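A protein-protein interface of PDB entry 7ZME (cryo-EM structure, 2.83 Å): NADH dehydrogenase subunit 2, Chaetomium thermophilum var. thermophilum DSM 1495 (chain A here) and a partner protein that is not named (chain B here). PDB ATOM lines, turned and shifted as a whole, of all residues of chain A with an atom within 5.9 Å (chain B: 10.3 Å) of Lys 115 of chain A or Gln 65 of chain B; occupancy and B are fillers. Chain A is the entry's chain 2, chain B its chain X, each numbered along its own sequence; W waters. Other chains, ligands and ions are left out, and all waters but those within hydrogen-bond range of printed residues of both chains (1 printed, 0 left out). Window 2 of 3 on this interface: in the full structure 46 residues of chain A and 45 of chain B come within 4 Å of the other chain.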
ATOM      1  N   ASP A  20      35.670  23.993 -21.599  1.00  0.00           N
ATOM      2  CA  ASP A  20      34.790  23.130 -22.425  1.00  0.00           C
ATOM      3  C   ASP A  20      35.625  22.080 -23.167  1.00  0.00           C
ATOM      4  O   ASP A  20      35.027  21.176 -23.770  1.00  0.00           O
ATOM      5  CB  ASP A  20      33.933  23.975 -23.371  1.00  0.00           C
ATOM      6  CG  ASP A  20      34.689  24.816 -24.378  1.00  0.00           C
ATOM      7  OD1 ASP A  20      35.910  24.948 -24.234  1.00  0.00           O
ATOM      8  OD2 ASP A  20      34.038  25.327 -25.305  1.00  0.00           O
ATOM      9  N   ILE A  23      36.359  17.490 -21.659  1.00  0.00           N
ATOM     10  CA  ILE A  23      35.748  16.222 -22.146  1.00  0.00           C
ATOM     11  C   ILE A  23      36.549  15.685 -23.329  1.00  0.00           C
ATOM     12  O   ILE A  23      36.724  14.463 -23.382  1.00  0.00           O
ATOM     13  CB  ILE A  23      34.256  16.449 -22.490  1.00  0.00           C
ATOM     14  CG1 ILE A  23      33.520  15.162 -22.866  1.00  0.00           C
ATOM     15  CG2 ILE A  23      34.073  17.537 -23.536  1.00  0.00           C
ATOM     16  CD1 ILE A  23      32.442  14.772 -21.887  1.00  0.00           C
ATOM     17  N   TYR A  85      29.369  12.157 -20.665  1.00  0.00           N
ATOM     18  CA  TYR A  85      28.423  12.743 -19.681  1.00  0.00           C
ATOM     19  C   TYR A  85      27.670  11.618 -18.973  1.00  0.00           C
ATOM     20  O   TYR A  85      27.384  10.612 -19.616  1.00  0.00           O
ATOM     21  CB  TYR A  85      27.524  13.776 -20.368  1.00  0.00           C
ATOM     22  CG  TYR A  85      28.250  14.990 -20.881  1.00  0.00           C
ATOM     23  CD1 TYR A  85      28.734  15.951 -20.010  1.00  0.00           C
ATOM     24  CD2 TYR A  85      28.451  15.179 -22.236  1.00  0.00           C
ATOM     25  CE1 TYR A  85      29.409  17.066 -20.472  1.00  0.00           C
ATOM     26  CE2 TYR A  85      29.119  16.292 -22.715  1.00  0.00           C
ATOM     27  CZ  TYR A  85      29.598  17.238 -21.829  1.00  0.00           C
ATOM     28  OH  TYR A  85      30.258  18.335 -22.296  1.00  0.00           O
ATOM     29  N   ARG A 109      20.323  20.411 -22.940  1.00  0.00           N
ATOM     30  CA  ARG A 109      20.893  19.272 -22.178  1.00  0.00           C
ATOM     31  C   ARG A 109      21.853  19.725 -21.087  1.00  0.00           C
ATOM     32  O   ARG A 109      22.374  18.843 -20.408  1.00  0.00           O
ATOM     33  CB  ARG A 109      21.588  18.284 -23.119  1.00  0.00           C
ATOM     34  CG  ARG A 109      22.410  18.889 -24.243  1.00  0.00           C
ATOM     35  CD  ARG A 109      23.046  17.736 -24.993  1.00  0.00           C
ATOM     36  NE  ARG A 109      22.386  17.403 -26.244  1.00  0.00           N
ATOM     37  CZ  ARG A 109      22.704  16.366 -27.009  1.00  0.00           C
ATOM     38  NH1 ARG A 109      23.666  15.540 -26.638  1.00  0.00           N
ATOM     39  NH2 ARG A 109      22.054  16.153 -28.137  1.00  0.00           N
ATOM     40  N   THR A 110      22.028  21.031 -20.867  1.00  0.00           N
ATOM     41  CA  THR A 110      23.083  21.435 -19.905  1.00  0.00           C
ATOM     42  C   THR A 110      22.798  20.835 -18.533  1.00  0.00           C
ATOM     43  O   THR A 110      23.713  20.224 -17.966  1.00  0.00           O
ATOM     44  CB  THR A 110      23.206  22.957 -19.799  1.00  0.00           C
ATOM     45  OG1 THR A 110      23.283  23.476 -21.126  1.00  0.00           O
ATOM     46  CG2 THR A 110      24.410  23.407 -19.001  1.00  0.00           C
ATOM     47  N   LYS A 111      21.563  20.971 -18.043  1.00  0.00           N
ATOM     48  CA  LYS A 111      21.181  20.384 -16.734  1.00  0.00           C
ATOM     49  C   LYS A 111      21.095  18.852 -16.787  1.00  0.00           C
ATOM     50  O   LYS A 111      21.601  18.220 -15.855  1.00  0.00           O
ATOM     51  CB  LYS A 111      19.902  21.058 -16.244  1.00  0.00           C
ATOM     52  CG  LYS A 111      19.911  22.577 -16.311  1.00  0.00           C
ATOM     53  CD  LYS A 111      18.558  23.192 -16.032  1.00  0.00           C
ATOM     54  CE  LYS A 111      18.560  24.700 -16.151  1.00  0.00           C
ATOM     55  NZ  LYS A 111      19.600  25.311 -15.292  1.00  0.00           N
ATOM     56  N   ILE A 113      22.606  16.638 -18.652  1.00  0.00           N
ATOM     57  CA  ILE A 113      23.919  15.946 -18.784  1.00  0.00           C
ATOM     58  C   ILE A 113      24.928  16.470 -17.755  1.00  0.00           C
ATOM     59  O   ILE A 113      26.013  15.878 -17.680  1.00  0.00           O
ATOM     60  CB  ILE A 113      24.447  16.069 -20.226  1.00  0.00           C
ATOM     61  CG1 ILE A 113      25.086  17.430 -20.510  1.00  0.00           C
ATOM     62  CG2 ILE A 113      23.367  15.703 -21.233  1.00  0.00           C
ATOM     63  CD1 ILE A 113      25.520  17.622 -21.939  1.00  0.00           C
ATOM     64  N   ASN A 114      24.599  17.519 -16.996  1.00  0.00           N
ATOM     65  CA  ASN A 114      25.573  18.160 -16.069  1.00  0.00           C
ATOM     66  C   ASN A 114      26.824  18.555 -16.861  1.00  0.00           C
ATOM     67  O   ASN A 114      27.929  18.184 -16.441  1.00  0.00           O
ATOM     68  CB  ASN A 114      25.845  17.309 -14.828  1.00  0.00           C
ATOM     69  CG  ASN A 114      26.407  18.109 -13.673  1.00  0.00           C
ATOM     70  OD1 ASN A 114      26.357  19.336 -13.675  1.00  0.00           O
ATOM     71  ND2 ASN A 114      26.944  17.421 -12.680  1.00  0.00           N
ATOM     72  N   LYS A 115      26.654  19.332 -17.932  1.00  0.00           N
ATOM     73  CA  LYS A 115      27.781  19.704 -18.827  1.00  0.00           C
ATOM     74  C   LYS A 115      28.829  20.495 -18.052  1.00  0.00           C
ATOM     75  O   LYS A 115      30.031  20.290 -18.299  1.00  0.00           O
ATOM     76  CB  LYS A 115      27.277  20.519 -20.021  1.00  0.00           C
ATOM     77  CG  LYS A 115      28.363  21.088 -20.921  1.00  0.00           C
ATOM     78  CD  LYS A 115      27.868  21.488 -22.286  1.00  0.00           C
ATOM     79  CE  LYS A 115      26.790  22.548 -22.249  1.00  0.00           C
ATOM     80  NZ  LYS A 115      26.371  22.935 -23.616  1.00  0.00           N
ATOM     81  N   MET A 116      28.385  21.354 -17.145  1.00  0.00           N
ATOM     82  CA  MET A 116      29.327  22.224 -16.410  1.00  0.00           C
ATOM     83  C   MET A 116      29.529  21.682 -14.995  1.00  0.00           C
ATOM     84  O   MET A 116      29.558  22.491 -14.064  1.00  0.00           O
ATOM     85  CB  MET A 116      28.841  23.671 -16.414  1.00  0.00           C
ATOM     86  CG  MET A 116      28.616  24.207 -17.811  1.00  0.00           C
ATOM     87  SD  MET A 116      27.622  25.712 -17.812  1.00  0.00           S
ATOM     88  CE  MET A 116      27.675  26.145 -19.549  1.00  0.00           C
ATOM     89  N   GLY A 117      29.666  20.360 -14.849  1.00  0.00           N
ATOM     90  CA  GLY A 117      30.021  19.777 -13.544  1.00  0.00           C
ATOM     91  C   GLY A 117      31.512  19.875 -13.308  1.00  0.00           C
ATOM     92  O   GLY A 117      32.230  20.132 -14.275  1.00  0.00           O
ATOM     93  N   MET A 120      33.858  17.733 -15.236  1.00  0.00           N
ATOM     94  CA  MET A 120      33.846  18.064 -16.684  1.00  0.00           C
ATOM     95  C   MET A 120      34.545  19.395 -16.970  1.00  0.00           C
ATOM     96  O   MET A 120      34.503  19.829 -18.122  1.00  0.00           O
ATOM     97  CB  MET A 120      32.395  18.147 -17.162  1.00  0.00           C
ATOM     98  CG  MET A 120      31.654  16.824 -17.077  1.00  0.00           C
ATOM     99  SD  MET A 120      32.449  15.503 -18.038  1.00  0.00           S
ATOM    100  CE  MET A 120      31.300  14.162 -17.760  1.00  0.00           C
ATOM    101  N   LYS A 121      35.176  20.021 -15.977  1.00  0.00           N
ATOM    102  CA  LYS A 121      35.733  21.381 -16.202  1.00  0.00           C
ATOM    103  C   LYS A 121      37.226  21.450 -15.857  1.00  0.00           C
ATOM    104  O   LYS A 121      37.842  22.465 -16.211  1.00  0.00           O
ATOM    105  CB  LYS A 121      34.912  22.426 -15.438  1.00  0.00           C
ATOM    106  CG  LYS A 121      33.491  22.650 -15.932  1.00  0.00           C
ATOM    107  CD  LYS A 121      32.931  23.999 -15.546  1.00  0.00           C
ATOM    108  CE  LYS A 121      33.023  24.294 -14.065  1.00  0.00           C
ATOM    109  NZ  LYS A 121      32.161  23.399 -13.259  1.00  0.00           N
ATOM    110  N   MET B  58      33.174   9.071 -31.726  1.00  0.00           N
ATOM    111  CA  MET B  58      32.691   9.441 -30.374  1.00  0.00           C
ATOM    112  C   MET B  58      31.889  10.733 -30.511  1.00  0.00           C
ATOM    113  O   MET B  58      30.872  10.856 -29.829  1.00  0.00           O
ATOM    114  CB  MET B  58      33.836   9.636 -29.375  1.00  0.00           C
ATOM    115  CG  MET B  58      34.431   8.364 -28.810  1.00  0.00           C
ATOM    116  SD  MET B  58      36.166   8.629 -28.334  1.00  0.00           S
ATOM    117  CE  MET B  58      36.218   7.830 -26.733  1.00  0.00           C
ATOM    118  N   GLU B  59      32.346  11.653 -31.357  1.00  0.00           N
ATOM    119  CA  GLU B  59      31.637  12.935 -31.600  1.00  0.00           C
ATOM    120  C   GLU B  59      30.267  12.692 -32.234  1.00  0.00           C
ATOM    121  O   GLU B  59      29.321  13.388 -31.847  1.00  0.00           O
ATOM    122  CB  GLU B  59      32.490  13.823 -32.502  1.00  0.00           C
ATOM    123  CG  GLU B  59      31.891  15.186 -32.789  1.00  0.00           C
ATOM    124  CD  GLU B  59      31.952  16.213 -31.669  1.00  0.00           C
ATOM    125  OE1 GLU B  59      32.166  15.824 -30.504  1.00  0.00           O
ATOM    126  OE2 GLU B  59      31.795  17.407 -31.972  1.00  0.00           O
ATOM    127  N   ARG B  60      30.180  11.794 -33.216  1.00  0.00           N
ATOM    128  CA  ARG B  60      28.881  11.597 -33.900  1.00  0.00           C
ATOM    129  C   ARG B  60      27.878  10.968 -32.934  1.00  0.00           C
ATOM    130  O   ARG B  60      26.754  11.490 -32.825  1.00  0.00           O
ATOM    131  CB  ARG B  60      29.068  10.770 -35.170  1.00  0.00           C
ATOM    132  CG  ARG B  60      27.789  10.473 -35.939  1.00  0.00           C
ATOM    133  CD  ARG B  60      26.976  11.706 -36.288  1.00  0.00           C
ATOM    134  NE  ARG B  60      27.721  12.745 -36.984  1.00  0.00           N
ATOM    135  CZ  ARG B  60      27.819  12.847 -38.305  1.00  0.00           C
ATOM    136  NH1 ARG B  60      27.221  11.963 -39.083  1.00  0.00           N
ATOM    137  NH2 ARG B  60      28.515  13.832 -38.841  1.00  0.00           N
ATOM    138  N   ILE B  61      28.272   9.904 -32.244  1.00  0.00           N
ATOM    139  CA  ILE B  61      27.300   9.193 -31.370  1.00  0.00           C
ATOM    140  C   ILE B  61      27.028   9.999 -30.102  1.00  0.00           C
ATOM    141  O   ILE B  61      25.857  10.067 -29.684  1.00  0.00           O
ATOM    142  CB  ILE B  61      27.775   7.757 -31.098  1.00  0.00           C
ATOM    143  CG1 ILE B  61      28.066   7.029 -32.412  1.00  0.00           C
ATOM    144  CG2 ILE B  61      26.777   6.998 -30.237  1.00  0.00           C
ATOM    145  CD1 ILE B  61      28.762   5.707 -32.243  1.00  0.00           C
ATOM    146  N   SER B  62      28.072  10.582 -29.514  1.00  0.00           N
ATOM    147  CA  SER B  62      27.916  11.282 -28.215  1.00  0.00           C
ATOM    148  C   SER B  62      28.544  12.665 -28.321  1.00  0.00           C
ATOM    149  O   SER B  62      29.680  12.827 -27.887  1.00  0.00           O
ATOM    150  CB  SER B  62      28.508  10.464 -27.104  1.00  0.00           C
ATOM    151  OG  SER B  62      27.893   9.194 -27.048  1.00  0.00           O
ATOM    152  N   PRO B  63      27.846  13.705 -28.848  1.00  0.00           N
ATOM    153  CA  PRO B  63      28.476  15.014 -29.033  1.00  0.00           C
ATOM    154  C   PRO B  63      29.017  15.604 -27.721  1.00  0.00           C
ATOM    155  O   PRO B  63      28.313  15.589 -26.743  1.00  0.00           O
ATOM    156  CB  PRO B  63      27.373  15.874 -29.655  1.00  0.00           C
ATOM    157  CG  PRO B  63      26.416  14.885 -30.257  1.00  0.00           C
ATOM    158  CD  PRO B  63      26.428  13.745 -29.269  1.00  0.00           C
ATOM    159  N   SER B  64      30.237  16.126 -27.740  1.00  0.00           N
ATOM    160  CA  SER B  64      30.878  16.711 -26.537  1.00  0.00           C
ATOM    161  C   SER B  64      30.200  18.009 -26.098  1.00  0.00           C
ATOM    162  O   SER B  64      30.409  18.379 -24.943  1.00  0.00           O
ATOM    163  CB  SER B  64      32.335  16.926 -26.806  1.00  0.00           C
ATOM    164  OG  SER B  64      32.524  17.516 -28.085  1.00  0.00           O
ATOM    165  N   GLN B  65      29.486  18.695 -27.001  1.00  0.00           N
ATOM    166  CA  GLN B  65      28.812  19.995 -26.708  1.00  0.00           C
ATOM    167  C   GLN B  65      29.865  21.091 -26.549  1.00  0.00           C
ATOM    168  O   GLN B  65      29.611  22.035 -25.799  1.00  0.00           O
ATOM    169  CB  GLN B  65      27.831  19.898 -25.533  1.00  0.00           C
ATOM    170  CG  GLN B  65      26.869  18.722 -25.611  1.00  0.00           C
ATOM    171  CD  GLN B  65      25.951  18.794 -26.805  1.00  0.00           C
ATOM    172  OE1 GLN B  65      25.735  17.809 -27.503  1.00  0.00           O
ATOM    173  NE2 GLN B  65      25.400  19.972 -27.047  1.00  0.00           N
ATOM    174  N   VAL B  66      31.005  20.956 -27.221  1.00  0.00           N
ATOM    175  CA  VAL B  66      32.116  21.954 -27.152  1.00  0.00           C
ATOM    176  C   VAL B  66      31.784  23.183 -28.003  1.00  0.00           C
ATOM    177  O   VAL B  66      30.938  23.064 -28.905  1.00  0.00           O
ATOM    178  CB  VAL B  66      33.463  21.317 -27.556  1.00  0.00           C
ATOM    179  CG1 VAL B  66      33.493  20.897 -29.017  1.00  0.00           C
ATOM    180  CG2 VAL B  66      34.669  22.174 -27.207  1.00  0.00           C
ATOM    181  N   GLY B  67      32.417  24.323 -27.714  1.00  0.00           N
ATOM    182  CA  GLY B  67      32.238  25.556 -28.498  1.00  0.00           C
ATOM    183  C   GLY B  67      32.647  25.442 -29.949  1.00  0.00           C
ATOM    184  O   GLY B  67      33.109  24.364 -30.340  1.00  0.00           O
ATOM    185  N   ARG B  68      32.630  26.549 -30.689  1.00  0.00           N
ATOM    186  CA  ARG B  68      32.829  26.534 -32.161  1.00  0.00           C
ATOM    187  C   ARG B  68      34.184  26.005 -32.648  1.00  0.00           C
ATOM    188  O   ARG B  68      34.177  25.343 -33.703  1.00  0.00           O
ATOM    189  CB  ARG B  68      32.566  27.932 -32.720  1.00  0.00           C
ATOM    190  CG  ARG B  68      31.161  28.444 -32.444  1.00  0.00           C
ATOM    191  CD  ARG B  68      30.864  29.767 -33.124  1.00  0.00           C
ATOM    192  NE  ARG B  68      29.491  30.195 -32.896  1.00  0.00           N
ATOM    193  CZ  ARG B  68      28.468  29.902 -33.691  1.00  0.00           C
ATOM    194  NH1 ARG B  68      28.659  29.180 -34.781  1.00  0.00           N
ATOM    195  NH2 ARG B  68      27.256  30.338 -33.395  1.00  0.00           N
ATOM    196  N   GLY B  69      35.303  26.319 -32.004  1.00  0.00           N
ATOM    197  CA  GLY B  69      36.581  25.857 -32.597  1.00  0.00           C
ATOM    198  C   GLY B  69      37.250  24.683 -31.903  1.00  0.00           C
ATOM    199  O   GLY B  69      38.349  24.316 -32.342  1.00  0.00           O
ATOM    200  N   GLY B  70      36.635  24.129 -30.857  1.00  0.00           N
ATOM    201  CA  GLY B  70      37.263  23.071 -30.041  1.00  0.00           C
ATOM    202  C   GLY B  70      37.496  21.744 -30.721  1.00  0.00           C
ATOM    203  O   GLY B  70      38.539  21.146 -30.447  1.00  0.00           O
ATOM    204  N   PHE B  71      36.533  21.254 -31.504  1.00  0.00           N
ATOM    205  CA  PHE B  71      36.680  19.912 -32.123  1.00  0.00           C
ATOM    206  C   PHE B  71      37.834  19.945 -33.118  1.00  0.00           C
ATOM    207  O   PHE B  71      38.609  18.987 -33.137  1.00  0.00           O
ATOM    208  CB  PHE B  71      35.376  19.378 -32.712  1.00  0.00           C
ATOM    209  CG  PHE B  71      35.442  17.915 -33.065  1.00  0.00           C
ATOM    210  CD1 PHE B  71      35.632  16.960 -32.080  1.00  0.00           C
ATOM    211  CD2 PHE B  71      35.342  17.493 -34.380  1.00  0.00           C
ATOM    212  CE1 PHE B  71      35.713  15.616 -32.401  1.00  0.00           C
ATOM    213  CE2 PHE B  71      35.415  16.146 -34.699  1.00  0.00           C
ATOM    214  CZ  PHE B  71      35.602  15.212 -33.709  1.00  0.00           C
HETATM  215  O   HOH W   1      31.687  21.448 -23.779  1.00  0.00           O
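Among the printed residues, pairs that only touch across the chains: Asp 20 of chain A with Val 66 of chain B (3.6 Å), Ile 23 of chain A with Ser 64 of chain B (3.8 Å) and Lys 115 of chain A with Gln 65 of chain B (3.6 Å).
Printed residues of chain B within 4 Å of Arg 109 of chain A: Gln 65. Thr 110 of chain A touches none of the printed residues of chain B. No residue of chain B comes within 4 Å of Ile 113 of chain A. No residue of chain B comes within 4 Å of Asn 114 of chain A. Lys 115 of chain A touches one residue of chain B. No residue of chain B comes within 4 Å of Met 116 of chain A. No residue of chain B comes within 4 Å of Gly 117 of chain A. Printed residues of chain A within 4 Å of Ser 64 of chain B: Ile 23 and Tyr 85. Of the printed residues of chain A, Val 66 of chain B touches Asp 20 (3.6 Å). Phe 71 of chain B touches none of the printed residues of chain A. The nearest residue of chain B that does not touch Lys 115 of chain A is Ser 64 of chain B (4.8 Å). The nearest residue of chain A that does not touch Gln 65 of chain B is Ile 113 of chain A (4.1 Å). The nearest printed residue of chain A that does not touch Ser 64 of chain B is Lys 115 of chain A (4.8 Å).
O of Ser 64 of chain B lies within hydrogen-bond range of OH of Tyr 85 of chain A (2.7 Å). The side-chain amide oxygen (OE1) of Gln 65 of chain B lies within hydrogen-bond range of the guanidinium group (NH1) of Arg 109 of chain A (3.2 Å). The side-chain carboxylate of Asp 20 of chain A is in hydrogen-bond range of the backbone NH of Gly 67 of chain B.
The side-chain carboxylate (OE1) of Glu 59 of chain B lies within hydrogen-bond range of the side-chain hydroxyl (OG) of Ser 64 of chain B (3.0 Å). O of Pro 63 of chain B lies close to OE1 of Gln 65 of chain B (3.5 Å). N of Lys 115 of chain A is in hydrogen-bond range of O of Thr 110 of chain A (3.1 Å).
Water W1 bridges the backbone carbonyl oxygen of Gln 65 of chain B and the backbone carbonyl oxygen of Asp 20 of chain A.
Hydrophobic or aromatic side chains of chain A that line the printed part of chain B: Ile 23 and Tyr 85. Of the 14 printed residues of chain B, 4 touch a printed residue of chain A. Along chain B the printed residues that touch a printed residue of chain A span positions 64 to 67. Among the printed residues, 6 pairs touch across the chains.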
